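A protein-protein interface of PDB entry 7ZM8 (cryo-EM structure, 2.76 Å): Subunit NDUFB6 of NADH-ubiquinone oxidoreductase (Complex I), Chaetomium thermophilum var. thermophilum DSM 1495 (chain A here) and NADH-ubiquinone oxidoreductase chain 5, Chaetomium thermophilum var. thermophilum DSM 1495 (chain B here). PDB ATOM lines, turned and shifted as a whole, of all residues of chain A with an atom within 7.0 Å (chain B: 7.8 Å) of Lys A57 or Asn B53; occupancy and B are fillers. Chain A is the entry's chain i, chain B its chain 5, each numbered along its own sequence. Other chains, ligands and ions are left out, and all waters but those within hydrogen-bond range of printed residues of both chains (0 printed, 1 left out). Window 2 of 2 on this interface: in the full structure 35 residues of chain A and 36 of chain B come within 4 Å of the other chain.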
ATOM      1  N   VAL A  54      14.871  20.517  -1.805  1.00  0.00           N
ATOM      2  CA  VAL A  54      15.712  19.554  -1.107  1.00  0.00           C
ATOM      3  C   VAL A  54      16.488  18.739  -2.128  1.00  0.00           C
ATOM      4  O   VAL A  54      15.901  18.169  -3.054  1.00  0.00           O
ATOM      5  CB  VAL A  54      14.884  18.639  -0.190  1.00  0.00           C
ATOM      6  CG1 VAL A  54      15.766  17.583   0.433  1.00  0.00           C
ATOM      7  CG2 VAL A  54      14.235  19.458   0.895  1.00  0.00           C
ATOM      8  N   ARG A  55      17.805  18.687  -1.954  1.00  0.00           N
ATOM      9  CA  ARG A  55      18.692  17.903  -2.794  1.00  0.00           C
ATOM     10  C   ARG A  55      19.519  16.982  -1.917  1.00  0.00           C
ATOM     11  O   ARG A  55      19.957  17.373  -0.833  1.00  0.00           O
ATOM     12  CB  ARG A  55      19.623  18.791  -3.612  1.00  0.00           C
ATOM     13  CG  ARG A  55      18.937  19.617  -4.674  1.00  0.00           C
ATOM     14  CD  ARG A  55      19.859  20.689  -5.205  1.00  0.00           C
ATOM     15  NE  ARG A  55      19.255  21.412  -6.317  1.00  0.00           N
ATOM     16  CZ  ARG A  55      18.356  22.379  -6.176  1.00  0.00           C
ATOM     17  NH1 ARG A  55      17.855  22.978  -7.240  1.00  0.00           N
ATOM     18  NH2 ARG A  55      17.946  22.735  -4.973  1.00  0.00           N
ATOM     19  N   HIS A  56      19.773  15.770  -2.414  1.00  0.00           N
ATOM     20  CA  HIS A  56      20.599  14.778  -1.677  1.00  0.00           C
ATOM     21  C   HIS A  56      21.956  14.650  -2.367  1.00  0.00           C
ATOM     22  O   HIS A  56      22.713  13.744  -1.989  1.00  0.00           O
ATOM     23  CB  HIS A  56      19.869  13.430  -1.610  1.00  0.00           C
ATOM     24  CG  HIS A  56      18.523  13.499  -0.975  1.00  0.00           C
ATOM     25  ND1 HIS A  56      18.357  13.690   0.379  1.00  0.00           N
ATOM     26  CD2 HIS A  56      17.284  13.395  -1.499  1.00  0.00           C
ATOM     27  CE1 HIS A  56      17.071  13.708   0.662  1.00  0.00           C
ATOM     28  NE2 HIS A  56      16.391  13.526  -0.473  1.00  0.00           N
ATOM     29  N   LYS A  57      22.254  15.527  -3.325  1.00  0.00           N
ATOM     30  CA  LYS A  57      23.513  15.490  -4.045  1.00  0.00           C
ATOM     31  C   LYS A  57      23.842  16.899  -4.500  1.00  0.00           C
ATOM     32  O   LYS A  57      23.031  17.542  -5.170  1.00  0.00           O
ATOM     33  CB  LYS A  57      23.428  14.545  -5.244  1.00  0.00           C
ATOM     34  CG  LYS A  57      24.699  14.399  -6.036  1.00  0.00           C
ATOM     35  CD  LYS A  57      24.480  13.470  -7.213  1.00  0.00           C
ATOM     36  CE  LYS A  57      25.743  13.310  -8.039  1.00  0.00           C
ATOM     37  NZ  LYS A  57      25.521  12.417  -9.207  1.00  0.00           N
ATOM     38  N   MET A  58      24.989  17.368  -4.135  1.00  0.00           N
ATOM     39  CA  MET A  58      25.328  18.722  -4.539  1.00  0.00           C
ATOM     40  C   MET A  58      26.049  18.727  -5.878  1.00  0.00           C
ATOM     41  O   MET A  58      26.696  17.745  -6.249  1.00  0.00           O
ATOM     42  CB  MET A  58      26.200  19.399  -3.480  1.00  0.00           C
ATOM     43  CG  MET A  58      25.639  19.351  -2.071  1.00  0.00           C
ATOM     44  SD  MET A  58      24.327  20.565  -1.797  1.00  0.00           S
ATOM     45  CE  MET A  58      22.853  19.620  -2.173  1.00  0.00           C
ATOM     46  N   PRO A  59      25.938  19.820  -6.623  1.00  0.00           N
ATOM     47  CA  PRO A  59      26.565  19.882  -7.944  1.00  0.00           C
ATOM     48  C   PRO A  59      28.075  20.021  -7.854  1.00  0.00           C
ATOM     49  O   PRO A  59      28.647  20.310  -6.802  1.00  0.00           O
ATOM     50  CB  PRO A  59      25.937  21.127  -8.575  1.00  0.00           C
ATOM     51  CG  PRO A  59      25.522  21.957  -7.422  1.00  0.00           C
ATOM     52  CD  PRO A  59      25.108  21.004  -6.351  1.00  0.00           C
ATOM     53  N   GLU A  60      28.722  19.806  -8.994  1.00  0.00           N
ATOM     54  CA  GLU A  60      30.163  19.948  -9.078  1.00  0.00           C
ATOM     55  C   GLU A  60      30.558  21.425  -9.123  1.00  0.00           C
ATOM     56  O   GLU A  60      29.798  22.265  -9.608  1.00  0.00           O
ATOM     57  CB  GLU A  60      30.688  19.227 -10.313  1.00  0.00           C
ATOM     58  CG  GLU A  60      30.349  17.755 -10.334  1.00  0.00           C
ATOM     59  CD  GLU A  60      31.514  16.886  -9.925  1.00  0.00           C
ATOM     60  OE1 GLU A  60      32.656  17.389  -9.911  1.00  0.00           O
ATOM     61  OE2 GLU A  60      31.290  15.696  -9.621  1.00  0.00           O
ATOM     62  N   ARG A  63      30.799  22.715 -12.838  1.00  0.00           N
ATOM     63  CA  ARG A  63      29.788  22.197 -13.743  1.00  0.00           C
ATOM     64  C   ARG A  63      28.550  23.082 -13.716  1.00  0.00           C
ATOM     65  O   ARG A  63      28.044  23.430 -12.648  1.00  0.00           O
ATOM     66  CB  ARG A  63      29.456  20.756 -13.354  1.00  0.00           C
ATOM     67  CG  ARG A  63      28.386  20.087 -14.154  1.00  0.00           C
ATOM     68  CD  ARG A  63      28.719  20.044 -15.614  1.00  0.00           C
ATOM     69  NE  ARG A  63      27.719  19.268 -16.327  1.00  0.00           N
ATOM     70  CZ  ARG A  63      27.885  18.008 -16.697  1.00  0.00           C
ATOM     71  NH1 ARG A  63      26.917  17.363 -17.326  1.00  0.00           N
ATOM     72  NH2 ARG A  63      29.046  17.415 -16.496  1.00  0.00           N
ATOM     73  N   PHE A  64      28.080  23.458 -14.906  1.00  0.00           N
ATOM     74  CA  PHE A  64      27.001  24.428 -15.073  1.00  0.00           C
ATOM     75  C   PHE A  64      25.751  24.051 -14.293  1.00  0.00           C
ATOM     76  O   PHE A  64      25.125  23.024 -14.570  1.00  0.00           O
ATOM     77  CB  PHE A  64      26.662  24.571 -16.555  1.00  0.00           C
ATOM     78  CG  PHE A  64      25.475  25.442 -16.828  1.00  0.00           C
ATOM     79  CD1 PHE A  64      25.584  26.815 -16.784  1.00  0.00           C
ATOM     80  CD2 PHE A  64      24.254  24.887 -17.152  1.00  0.00           C
ATOM     81  CE1 PHE A  64      24.500  27.611 -17.045  1.00  0.00           C
ATOM     82  CE2 PHE A  64      23.171  25.681 -17.415  1.00  0.00           C
ATOM     83  CZ  PHE A  64      23.293  27.044 -17.362  1.00  0.00           C
ATOM     84  N   TYR A  65      25.371  24.880 -13.325  1.00  0.00           N
ATOM     85  CA  TYR A  65      24.241  24.584 -12.446  1.00  0.00           C
ATOM     86  C   TYR A  65      23.761  25.904 -11.865  1.00  0.00           C
ATOM     87  O   TYR A  65      24.115  26.276 -10.742  1.00  0.00           O
ATOM     88  CB  TYR A  65      24.657  23.620 -11.339  1.00  0.00           C
ATOM     89  CG  TYR A  65      23.533  22.939 -10.610  1.00  0.00           C
ATOM     90  CD1 TYR A  65      22.868  21.868 -11.180  1.00  0.00           C
ATOM     91  CD2 TYR A  65      23.112  23.384  -9.370  1.00  0.00           C
ATOM     92  CE1 TYR A  65      21.850  21.230 -10.522  1.00  0.00           C
ATOM     93  CE2 TYR A  65      22.081  22.762  -8.709  1.00  0.00           C
ATOM     94  CZ  TYR A  65      21.451  21.690  -9.289  1.00  0.00           C
ATOM     95  OH  TYR A  65      20.418  21.073  -8.633  1.00  0.00           O
ATOM     96  N   ARG A  68      22.898  27.156  -8.187  1.00  0.00           N
ATOM     97  CA  ARG A  68      23.919  27.454  -7.185  1.00  0.00           C
ATOM     98  C   ARG A  68      23.811  28.853  -6.620  1.00  0.00           C
ATOM     99  O   ARG A  68      24.344  29.117  -5.539  1.00  0.00           O
ATOM    100  CB  ARG A  68      25.314  27.303  -7.788  1.00  0.00           C
ATOM    101  CG  ARG A  68      25.808  25.886  -7.909  1.00  0.00           C
ATOM    102  CD  ARG A  68      27.271  25.897  -8.271  1.00  0.00           C
ATOM    103  NE  ARG A  68      27.464  26.437  -9.608  1.00  0.00           N
ATOM    104  CZ  ARG A  68      27.665  25.688 -10.684  1.00  0.00           C
ATOM    105  NH1 ARG A  68      27.715  24.371 -10.569  1.00  0.00           N
ATOM    106  NH2 ARG A  68      27.829  26.255 -11.870  1.00  0.00           N
ATOM    107  N   GLN A  73      20.347  25.625   0.451  1.00  0.00           N
ATOM    108  CA  GLN A  73      21.035  24.381   0.784  1.00  0.00           C
ATOM    109  C   GLN A  73      22.359  24.272   0.046  1.00  0.00           C
ATOM    110  O   GLN A  73      23.376  23.882   0.628  1.00  0.00           O
ATOM    111  CB  GLN A  73      20.151  23.179   0.465  1.00  0.00           C
ATOM    112  CG  GLN A  73      20.894  21.857   0.543  1.00  0.00           C
ATOM    113  CD  GLN A  73      20.039  20.672   0.185  1.00  0.00           C
ATOM    114  OE1 GLN A  73      18.888  20.819  -0.222  1.00  0.00           O
ATOM    115  NE2 GLN A  73      20.593  19.480   0.336  1.00  0.00           N
ATOM    116  N   ILE A  74      22.361  24.615  -1.241  1.00  0.00           N
ATOM    117  CA  ILE A  74      23.597  24.602  -2.014  1.00  0.00           C
ATOM    118  C   ILE A  74      24.519  25.714  -1.553  1.00  0.00           C
ATOM    119  O   ILE A  74      25.729  25.517  -1.416  1.00  0.00           O
ATOM    120  CB  ILE A  74      23.288  24.715  -3.517  1.00  0.00           C
ATOM    121  CG1 ILE A  74      22.590  23.452  -4.008  1.00  0.00           C
ATOM    122  CG2 ILE A  74      24.553  24.990  -4.315  1.00  0.00           C
ATOM    123  CD1 ILE A  74      22.134  23.548  -5.418  1.00  0.00           C
ATOM    124  N   ILE B  45      16.245  24.853 -18.543  1.00  0.00           N
ATOM    125  CA  ILE B  45      17.307  24.900 -17.547  1.00  0.00           C
ATOM    126  C   ILE B  45      17.194  23.725 -16.588  1.00  0.00           C
ATOM    127  O   ILE B  45      18.200  23.097 -16.237  1.00  0.00           O
ATOM    128  CB  ILE B  45      17.287  26.242 -16.797  1.00  0.00           C
ATOM    129  CG1 ILE B  45      17.199  27.412 -17.769  1.00  0.00           C
ATOM    130  CG2 ILE B  45      18.516  26.377 -15.927  1.00  0.00           C
ATOM    131  CD1 ILE B  45      16.848  28.718 -17.099  1.00  0.00           C
ATOM    132  N   ALA B  46      15.975  23.400 -16.152  1.00  0.00           N
ATOM    133  CA  ALA B  46      15.791  22.308 -15.202  1.00  0.00           C
ATOM    134  C   ALA B  46      16.182  20.962 -15.796  1.00  0.00           C
ATOM    135  O   ALA B  46      16.469  20.020 -15.051  1.00  0.00           O
ATOM    136  CB  ALA B  46      14.345  22.276 -14.716  1.00  0.00           C
ATOM    137  N   PHE B  47      16.185  20.842 -17.124  1.00  0.00           N
ATOM    138  CA  PHE B  47      16.677  19.618 -17.745  1.00  0.00           C
ATOM    139  C   PHE B  47      18.181  19.477 -17.554  1.00  0.00           C
ATOM    140  O   PHE B  47      18.677  18.386 -17.254  1.00  0.00           O
ATOM    141  CB  PHE B  47      16.314  19.600 -19.227  1.00  0.00           C
ATOM    142  CG  PHE B  47      16.415  18.243 -19.863  1.00  0.00           C
ATOM    143  CD1 PHE B  47      15.333  17.388 -19.870  1.00  0.00           C
ATOM    144  CD2 PHE B  47      17.593  17.825 -20.453  1.00  0.00           C
ATOM    145  CE1 PHE B  47      15.421  16.146 -20.451  1.00  0.00           C
ATOM    146  CE2 PHE B  47      17.686  16.587 -21.035  1.00  0.00           C
ATOM    147  CZ  PHE B  47      16.596  15.745 -21.036  1.00  0.00           C
ATOM    148  N   PHE B  48      18.923  20.569 -17.729  1.00  0.00           N
ATOM    149  CA  PHE B  48      20.343  20.564 -17.406  1.00  0.00           C
ATOM    150  C   PHE B  48      20.560  20.343 -15.915  1.00  0.00           C
ATOM    151  O   PHE B  48      21.418  19.551 -15.511  1.00  0.00           O
ATOM    152  CB  PHE B  48      20.966  21.884 -17.852  1.00  0.00           C
ATOM    153  CG  PHE B  48      21.363  21.909 -19.296  1.00  0.00           C
ATOM    154  CD1 PHE B  48      22.414  21.148 -19.754  1.00  0.00           C
ATOM    155  CD2 PHE B  48      20.682  22.708 -20.195  1.00  0.00           C
ATOM    156  CE1 PHE B  48      22.778  21.172 -21.084  1.00  0.00           C
ATOM    157  CE2 PHE B  48      21.039  22.738 -21.526  1.00  0.00           C
ATOM    158  CZ  PHE B  48      22.090  21.969 -21.971  1.00  0.00           C
ATOM    159  N   GLU B  49      19.788  21.047 -15.084  1.00  0.00           N
ATOM    160  CA  GLU B  49      19.832  20.890 -13.634  1.00  0.00           C
ATOM    161  C   GLU B  49      19.748  19.428 -13.217  1.00  0.00           C
ATOM    162  O   GLU B  49      20.680  18.876 -12.624  1.00  0.00           O
ATOM    163  CB  GLU B  49      18.664  21.663 -13.027  1.00  0.00           C
ATOM    164  CG  GLU B  49      18.685  23.173 -13.160  1.00  0.00           C
ATOM    165  CD  GLU B  49      19.779  23.839 -12.376  1.00  0.00           C
ATOM    166  OE1 GLU B  49      20.139  23.328 -11.315  1.00  0.00           O
ATOM    167  OE2 GLU B  49      20.277  24.882 -12.810  1.00  0.00           O
ATOM    168  N   VAL B  50      18.622  18.785 -13.518  1.00  0.00           N
ATOM    169  CA  VAL B  50      18.270  17.512 -12.902  1.00  0.00           C
ATOM    170  C   VAL B  50      18.883  16.347 -13.660  1.00  0.00           C
ATOM    171  O   VAL B  50      19.520  15.474 -13.064  1.00  0.00           O
ATOM    172  CB  VAL B  50      16.741  17.352 -12.812  1.00  0.00           C
ATOM    173  CG1 VAL B  50      16.390  16.053 -12.135  1.00  0.00           C
ATOM    174  CG2 VAL B  50      16.124  18.513 -12.062  1.00  0.00           C
ATOM    175  N   GLY B  51      18.691  16.321 -14.977  1.00  0.00           N
ATOM    176  CA  GLY B  51      19.026  15.126 -15.732  1.00  0.00           C
ATOM    177  C   GLY B  51      20.511  14.991 -15.996  1.00  0.00           C
ATOM    178  O   GLY B  51      21.104  13.938 -15.752  1.00  0.00           O
ATOM    179  N   PHE B  52      21.131  16.050 -16.505  1.00  0.00           N
ATOM    180  CA  PHE B  52      22.532  15.966 -16.897  1.00  0.00           C
ATOM    181  C   PHE B  52      23.457  15.909 -15.694  1.00  0.00           C
ATOM    182  O   PHE B  52      24.638  15.584 -15.840  1.00  0.00           O
ATOM    183  CB  PHE B  52      22.892  17.149 -17.789  1.00  0.00           C
ATOM    184  CG  PHE B  52      22.491  16.961 -19.216  1.00  0.00           C
ATOM    185  CD1 PHE B  52      22.890  15.841 -19.916  1.00  0.00           C
ATOM    186  CD2 PHE B  52      21.706  17.896 -19.855  1.00  0.00           C
ATOM    187  CE1 PHE B  52      22.519  15.664 -21.222  1.00  0.00           C
ATOM    188  CE2 PHE B  52      21.338  17.722 -21.165  1.00  0.00           C
ATOM    189  CZ  PHE B  52      21.744  16.605 -21.848  1.00  0.00           C
ATOM    190  N   ASN B  53      22.950  16.218 -14.508  1.00  0.00           N
ATOM    191  CA  ASN B  53      23.758  16.203 -13.302  1.00  0.00           C
ATOM    192  C   ASN B  53      23.329  15.137 -12.307  1.00  0.00           C
ATOM    193  O   ASN B  53      24.016  14.948 -11.299  1.00  0.00           O
ATOM    194  CB  ASN B  53      23.717  17.575 -12.630  1.00  0.00           C
ATOM    195  CG  ASN B  53      24.637  18.565 -13.297  1.00  0.00           C
ATOM    196  OD1 ASN B  53      25.856  18.507 -13.150  1.00  0.00           O
ATOM    197  ND2 ASN B  53      24.051  19.503 -14.020  1.00  0.00           N
ATOM    198  N   ASN B  54      22.228  14.433 -12.574  1.00  0.00           N
ATOM    199  CA  ASN B  54      21.704  13.396 -11.688  1.00  0.00           C
ATOM    200  C   ASN B  54      21.413  13.951 -10.300  1.00  0.00           C
ATOM    201  O   ASN B  54      21.780  13.366  -9.280  1.00  0.00           O
ATOM    202  CB  ASN B  54      22.663  12.210 -11.604  1.00  0.00           C
ATOM    203  CG  ASN B  54      21.970  10.927 -11.196  1.00  0.00           C
ATOM    204  OD1 ASN B  54      20.954  10.942 -10.502  1.00  0.00           O
ATOM    205  ND2 ASN B  54      22.535   9.804 -11.608  1.00  0.00           N
ATOM    206  N   ILE B  55      20.749  15.099 -10.262  1.00  0.00           N
ATOM    207  CA  ILE B  55      20.341  15.686  -8.992  1.00  0.00           C
ATOM    208  C   ILE B  55      18.823  15.787  -8.957  1.00  0.00           C
ATOM    209  O   ILE B  55      18.260  16.779  -9.433  1.00  0.00           O
ATOM    210  CB  ILE B  55      20.985  17.061  -8.764  1.00  0.00           C
ATOM    211  CG1 ILE B  55      22.501  16.977  -8.900  1.00  0.00           C
ATOM    212  CG2 ILE B  55      20.635  17.591  -7.392  1.00  0.00           C
ATOM    213  CD1 ILE B  55      23.184  18.319  -8.821  1.00  0.00           C
ATOM    214  N   PRO B  56      18.128  14.793  -8.415  1.00  0.00           N
ATOM    215  CA  PRO B  56      16.689  14.943  -8.187  1.00  0.00           C
ATOM    216  C   PRO B  56      16.398  16.070  -7.208  1.00  0.00           C
ATOM    217  O   PRO B  56      17.183  16.350  -6.300  1.00  0.00           O
ATOM    218  CB  PRO B  56      16.284  13.583  -7.616  1.00  0.00           C
ATOM    219  CG  PRO B  56      17.279  12.653  -8.181  1.00  0.00           C
ATOM    220  CD  PRO B  56      18.567  13.409  -8.186  1.00  0.00           C
ATOM    221  N   SER B  80      14.798  12.553 -13.577  1.00  0.00           N
ATOM    222  CA  SER B  80      15.125  12.501 -14.997  1.00  0.00           C
ATOM    223  C   SER B  80      13.883  12.306 -15.850  1.00  0.00           C
ATOM    224  O   SER B  80      13.801  12.831 -16.965  1.00  0.00           O
ATOM    225  CB  SER B  80      16.137  11.394 -15.266  1.00  0.00           C
ATOM    226  OG  SER B  80      17.363  11.662 -14.621  1.00  0.00           O
ATOM    227  N   ASN B 498      23.313   6.118 -18.342  1.00  0.00           N
ATOM    228  CA  ASN B 498      22.945   6.298 -16.947  1.00  0.00           C
ATOM    229  C   ASN B 498      22.087   7.542 -16.738  1.00  0.00           C
ATOM    230  O   ASN B 498      22.176   8.195 -15.698  1.00  0.00           O
ATOM    231  CB  ASN B 498      24.200   6.365 -16.083  1.00  0.00           C
ATOM    232  CG  ASN B 498      25.108   7.515 -16.464  1.00  0.00           C
ATOM    233  OD1 ASN B 498      25.050   8.026 -17.582  1.00  0.00           O
ATOM    234  ND2 ASN B 498      25.952   7.933 -15.531  1.00  0.00           N
ATOM    235  N   PHE B 499      21.252   7.890 -17.716  1.00  0.00           N
ATOM    236  CA  PHE B 499      20.433   9.086 -17.568  1.00  0.00           C
ATOM    237  C   PHE B 499      19.279   8.854 -16.606  1.00  0.00           C
ATOM    238  O   PHE B 499      18.869   9.773 -15.889  1.00  0.00           O
ATOM    239  CB  PHE B 499      19.907   9.554 -18.922  1.00  0.00           C
ATOM    240  CG  PHE B 499      19.525  11.003 -18.941  1.00  0.00           C
ATOM    241  CD1 PHE B 499      20.483  11.979 -19.123  1.00  0.00           C
ATOM    242  CD2 PHE B 499      18.214  11.390 -18.748  1.00  0.00           C
ATOM    243  CE1 PHE B 499      20.143  13.307 -19.124  1.00  0.00           C
ATOM    244  CE2 PHE B 499      17.868  12.717 -18.753  1.00  0.00           C
ATOM    245  CZ  PHE B 499      18.831  13.676 -18.940  1.00  0.00           C
ATOM    246  N   VAL B 501      19.195   6.641 -14.009  1.00  0.00           N
ATOM    247  CA  VAL B 501      19.793   5.760 -13.013  1.00  0.00           C
ATOM    248  C   VAL B 501      19.431   6.261 -11.620  1.00  0.00           C
ATOM    249  O   VAL B 501      19.951   5.775 -10.613  1.00  0.00           O
ATOM    250  CB  VAL B 501      21.317   5.669 -13.212  1.00  0.00           C
ATOM    251  CG1 VAL B 501      21.993   6.942 -12.778  1.00  0.00           C
ATOM    252  CG2 VAL B 501      21.896   4.447 -12.536  1.00  0.00           C
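Printed residues of chain A that touch a printed residue of chain B: Val A54, Arg A55, Lys A57, Pro A59, Arg A63, Phe A64 and Tyr A65. Hydrophobic or aromatic side chains of chain A within 4 Å of the printed part of chain B: Pro A59 and Tyr A65. Of the 16 printed residues of chain B, 6 touch a printed residue of chain A. Hydrophobic or aromatic side chains of chain B that line the printed part of chain A: Ile B55. Along chain B the printed residues that touch a printed residue of chain A span positions 49 to 56. Among the printed residues, no Asp or Glu carboxylate lies within 4 Å of a Lys or Arg side-chain nitrogen of the other chain.
The guanidinium group of Arg A55 is in hydrogen-bond range of the side-chain hydroxyl of Tyr A65. The side-chain amide nitrogen of Gln A73 is in hydrogen-bond range of the backbone carbonyl oxygen of Arg A55. O of Arg A63 lies within hydrogen-bond range of NH2 of Arg A68 (2.9 Å). The backbone NH of Phe B52 lies within hydrogen-bond range of the backbone carbonyl oxygen of Phe B47. The backbone carbonyl oxygen of Phe B48 sits at hydrogen-bond distance from the side-chain amide nitrogen of Asn B53. The backbone carbonyl oxygen (O) of Val B50 sits at hydrogen-bond distance from the backbone NH (N) of Ile B55.
Pro B56 touches Val A54. CG2 of Ile B55 touches CG of Arg A55 (3.8 Å). Lys A57 touches Asn B53. CD of Lys A57 touches O of Asn B54, at 3.4 Å. Lys A57 touches Ile B55 (O to CG2, 3.3 Å). Ile B55 touches Pro A59. OD1 of Asn B53 touches CG of Arg A63, at 3.1 Å. O of Phe A64 touches ND2 of Asn B53 (3.7 Å). Tyr A65 touches Asn B53. Tyr A65 touches Ile B55.
Lys A57 touches three residues of chain B. Of the printed residues of chain B, Arg A63 touches Phe B52 and Asn B53. Of the printed residues of chain A, Phe B52 touches Arg A63. The nearest residue of chain B that does not touch Lys A57 is Pro B56 (5.8 Å). The nearest printed residue of chain B that does not touch Phe A64 is Phe B48 (4.4 Å).
The guanidinium group of Arg A63 lies within hydrogen-bond range of the backbone carbonyl oxygen of Phe B52 (3.3 Å).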
